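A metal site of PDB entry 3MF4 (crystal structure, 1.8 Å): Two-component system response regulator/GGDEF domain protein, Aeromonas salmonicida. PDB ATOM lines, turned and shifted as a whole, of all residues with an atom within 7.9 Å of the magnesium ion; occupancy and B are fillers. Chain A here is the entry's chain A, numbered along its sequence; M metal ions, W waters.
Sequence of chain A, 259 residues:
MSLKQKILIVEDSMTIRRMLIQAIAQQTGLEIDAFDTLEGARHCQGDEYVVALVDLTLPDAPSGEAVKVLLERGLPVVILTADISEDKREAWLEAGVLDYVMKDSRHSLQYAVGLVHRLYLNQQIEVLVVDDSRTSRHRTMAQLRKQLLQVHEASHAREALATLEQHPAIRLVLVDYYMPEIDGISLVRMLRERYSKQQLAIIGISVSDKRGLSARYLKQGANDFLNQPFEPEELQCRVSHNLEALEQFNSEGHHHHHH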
ATOM      1  N   VAL A 130     -23.003  -3.625  25.638  1.00  0.00           N
ATOM      2  CA  VAL A 130     -22.221  -2.687  24.822  1.00  0.00           C
ATOM      3  C   VAL A 130     -22.791  -2.679  23.406  1.00  0.00           C
ATOM      4  O   VAL A 130     -22.715  -3.683  22.696  1.00  0.00           O
ATOM      5  CB  VAL A 130     -20.699  -3.032  24.761  1.00  0.00           C
ATOM      6  CG1 VAL A 130     -19.916  -1.881  24.161  1.00  0.00           C
ATOM      7  CG2 VAL A 130     -20.128  -3.463  26.096  1.00  0.00           C
ATOM      8  N   ASP A 131     -23.360  -1.543  22.992  1.00  0.00           N
ATOM      9  CA  ASP A 131     -24.124  -1.513  21.741  1.00  0.00           C
ATOM     10  C   ASP A 131     -24.298  -0.060  21.342  1.00  0.00           C
ATOM     11  O   ASP A 131     -24.677   0.773  22.178  1.00  0.00           O
ATOM     12  CB  ASP A 131     -25.499  -2.168  21.963  1.00  0.00           C
ATOM     13  CG  ASP A 131     -26.227  -2.477  20.660  1.00  0.00           C
ATOM     14  OD1 ASP A 131     -25.946  -1.856  19.615  1.00  0.00           O
ATOM     15  OD2 ASP A 131     -27.144  -3.346  20.700  1.00  0.00           O
ATOM     16  N   ASP A 132     -23.952   0.255  20.108  1.00  0.00           N
ATOM     17  CA  ASP A 132     -24.056   1.636  19.593  1.00  0.00           C
ATOM     18  C   ASP A 132     -25.453   1.996  19.095  1.00  0.00           C
ATOM     19  O   ASP A 132     -25.706   3.175  18.824  1.00  0.00           O
ATOM     20  CB  ASP A 132     -23.045   1.906  18.504  1.00  0.00           C
ATOM     21  CG  ASP A 132     -23.304   1.097  17.256  1.00  0.00           C
ATOM     22  OD1 ASP A 132     -23.649  -0.091  17.394  1.00  0.00           O
ATOM     23  OD2 ASP A 132     -23.123   1.641  16.166  1.00  0.00           O
ATOM     24  N   SER A 133     -26.328   0.990  18.975  1.00  0.00           N
ATOM     25  CA  SER A 133     -27.740   1.230  18.664  1.00  0.00           C
ATOM     26  C   SER A 133     -28.559   1.388  19.954  1.00  0.00           C
ATOM     27  O   SER A 133     -28.689   0.434  20.728  1.00  0.00           O
ATOM     28  CB  SER A 133     -28.320   0.099  17.808  1.00  0.00           C
ATOM     29  OG  SER A 133     -29.755   0.117  17.811  1.00  0.00           O
ATOM     30  N   SER A 136     -31.479  -1.104  20.205  1.00  0.00           N
ATOM     31  CA  SER A 136     -30.976  -2.448  20.568  1.00  0.00           C
ATOM     32  C   SER A 136     -30.495  -2.495  22.009  1.00  0.00           C
ATOM     33  O   SER A 136     -30.801  -3.437  22.754  1.00  0.00           O
ATOM     34  CB  SER A 136     -29.825  -2.840  19.624  1.00  0.00           C
ATOM     35  OG  SER A 136     -30.325  -3.027  18.309  1.00  0.00           O
ATOM     36  N   SER A 155     -22.398   2.711  25.119  1.00  0.00           N
ATOM     37  CA  SER A 155     -22.715   2.930  23.712  1.00  0.00           C
ATOM     38  C   SER A 155     -21.505   2.880  22.788  1.00  0.00           C
ATOM     39  O   SER A 155     -21.607   3.308  21.641  1.00  0.00           O
ATOM     40  CB  SER A 155     -23.392   4.295  23.522  1.00  0.00           C
ATOM     41  OG  SER A 155     -24.319   4.564  24.546  1.00  0.00           O
ATOM     42  N   ASP A 176     -21.835  -5.961  21.052  1.00  0.00           N
ATOM     43  CA  ASP A 176     -22.345  -5.727  19.678  1.00  0.00           C
ATOM     44  C   ASP A 176     -21.218  -5.749  18.630  1.00  0.00           C
ATOM     45  O   ASP A 176     -20.116  -5.333  18.913  1.00  0.00           O
ATOM     46  CB  ASP A 176     -23.149  -4.413  19.650  1.00  0.00           C
ATOM     47  CG  ASP A 176     -23.617  -4.059  18.258  1.00  0.00           C
ATOM     48  OD1 ASP A 176     -24.299  -4.900  17.630  1.00  0.00           O
ATOM     49  OD2 ASP A 176     -23.285  -2.952  17.759  1.00  0.00           O
ATOM     50  N   TYR A 177     -21.489  -6.271  17.430  1.00  0.00           N
ATOM     51  CA  TYR A 177     -20.441  -6.512  16.456  1.00  0.00           C
ATOM     52  C   TYR A 177     -19.877  -5.284  15.752  1.00  0.00           C
ATOM     53  O   TYR A 177     -18.657  -5.145  15.570  1.00  0.00           O
ATOM     54  CB  TYR A 177     -20.895  -7.553  15.423  1.00  0.00           C
ATOM     55  CG  TYR A 177     -22.153  -7.219  14.670  1.00  0.00           C
ATOM     56  CD1 TYR A 177     -22.097  -6.547  13.448  1.00  0.00           C
ATOM     57  CD2 TYR A 177     -23.401  -7.631  15.137  1.00  0.00           C
ATOM     58  CE1 TYR A 177     -23.254  -6.258  12.730  1.00  0.00           C
ATOM     59  CE2 TYR A 177     -24.562  -7.338  14.427  1.00  0.00           C
ATOM     60  CZ  TYR A 177     -24.480  -6.660  13.224  1.00  0.00           C
ATOM     61  OH  TYR A 177     -25.627  -6.380  12.525  1.00  0.00           O
ATOM     62  N   TYR A 178     -20.764  -4.378  15.354  1.00  0.00           N
ATOM     63  CA  TYR A 178     -20.341  -3.196  14.623  1.00  0.00           C
ATOM     64  C   TYR A 178     -20.611  -1.925  15.429  1.00  0.00           C
ATOM     65  O   TYR A 178     -21.770  -1.619  15.718  1.00  0.00           O
ATOM     66  CB  TYR A 178     -21.035  -3.115  13.267  1.00  0.00           C
ATOM     67  CG  TYR A 178     -20.618  -1.891  12.483  1.00  0.00           C
ATOM     68  CD1 TYR A 178     -19.400  -1.857  11.839  1.00  0.00           C
ATOM     69  CD2 TYR A 178     -21.432  -0.752  12.437  1.00  0.00           C
ATOM     70  CE1 TYR A 178     -18.985  -0.722  11.133  1.00  0.00           C
ATOM     71  CE2 TYR A 178     -21.018   0.402  11.747  1.00  0.00           C
ATOM     72  CZ  TYR A 178     -19.794   0.400  11.096  1.00  0.00           C
ATOM     73  OH  TYR A 178     -19.363   1.507  10.419  1.00  0.00           O
ATOM     74  N   MET A 179     -19.539  -1.206  15.757  1.00  0.00           N
ATOM     75  CA  MET A 179     -19.628   0.036  16.510  1.00  0.00           C
ATOM     76  C   MET A 179     -18.528   0.983  16.023  1.00  0.00           C
ATOM     77  O   MET A 179     -17.506   0.517  15.522  1.00  0.00           O
ATOM     78  CB  MET A 179     -19.455  -0.237  18.015  1.00  0.00           C
ATOM     79  CG  MET A 179     -20.373  -1.306  18.609  1.00  0.00           C
ATOM     80  SD  MET A 179     -20.116  -1.399  20.560  1.00  0.00           S
ATOM     81  CE  MET A 179     -18.418  -2.355  20.490  1.00  0.00           C
ATOM     82  N   PRO A 180     -18.707   2.307  16.206  1.00  0.00           N
ATOM     83  CA  PRO A 180     -17.707   3.293  15.744  1.00  0.00           C
ATOM     84  C   PRO A 180     -16.369   3.062  16.444  1.00  0.00           C
ATOM     85  O   PRO A 180     -16.342   2.704  17.638  1.00  0.00           O
ATOM     86  CB  PRO A 180     -18.317   4.649  16.189  1.00  0.00           C
ATOM     87  CG  PRO A 180     -19.768   4.371  16.422  1.00  0.00           C
ATOM     88  CD  PRO A 180     -19.848   2.954  16.888  1.00  0.00           C
ATOM     89  N   GLY A 184     -16.859  -4.934  17.565  1.00  0.00           N
ATOM     90  CA  GLY A 184     -17.024  -5.982  18.566  1.00  0.00           C
ATOM     91  C   GLY A 184     -15.842  -6.915  18.749  1.00  0.00           C
ATOM     92  O   GLY A 184     -15.398  -7.136  19.864  1.00  0.00           O
ATOM     93  N   GLN A 228     -28.765 -11.722  16.427  1.00  0.00           N
ATOM     94  CA  GLN A 228     -29.868 -10.785  16.320  1.00  0.00           C
ATOM     95  C   GLN A 228     -30.657 -11.049  15.055  1.00  0.00           C
ATOM     96  O   GLN A 228     -30.077 -11.428  14.049  1.00  0.00           O
ATOM     97  CB  GLN A 228     -29.364  -9.340  16.319  1.00  0.00           C
ATOM     98  CG  GLN A 228     -29.637  -8.610  17.601  1.00  0.00           C
ATOM     99  CD  GLN A 228     -28.672  -7.478  17.823  1.00  0.00           C
ATOM    100  OE1 GLN A 228     -27.780  -7.237  17.005  1.00  0.00           O
ATOM    101  NE2 GLN A 228     -28.821  -6.767  18.945  1.00  0.00           N
HETATM  102 MG    MG M   1     -23.764  -1.744  16.133  1.00  0.00          MG
HETATM  103  O   HOH W   1     -25.685  -1.931  16.725  1.00  0.00           O
HETATM  104  O   HOH W   2     -23.940  -3.596  15.254  1.00  0.00           O
HETATM  105  O   HOH W   3     -24.265  -0.737  14.722  1.00  0.00           O
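Of the 13 residues printed, 3 come within 4 Å of the magnesium ion. The nearest printed residue that does not touch the magnesium ion is Asp 131 (4.1 Å).
The magnesium ion is bound by water W3, water W1, the backbone carbonyl oxygen (O) of Tyr 178, water W2, the side-chain carboxylate (OD2) of Asp 176 and the side-chain carboxylate (OD1) of Asp 132.
Water W2 bridges the side-chain carboxylate of Asp 176 (2.7 Å) and the backbone NH of Tyr 178 (3.3 Å). Water W1 bridges OD1 of Asp 131 and OD1 of Asp 176.
The backbone carbonyl oxygen (O) of Val 130 lies within hydrogen-bond range of the backbone NH (N) of Asp 176 (2.9 Å).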
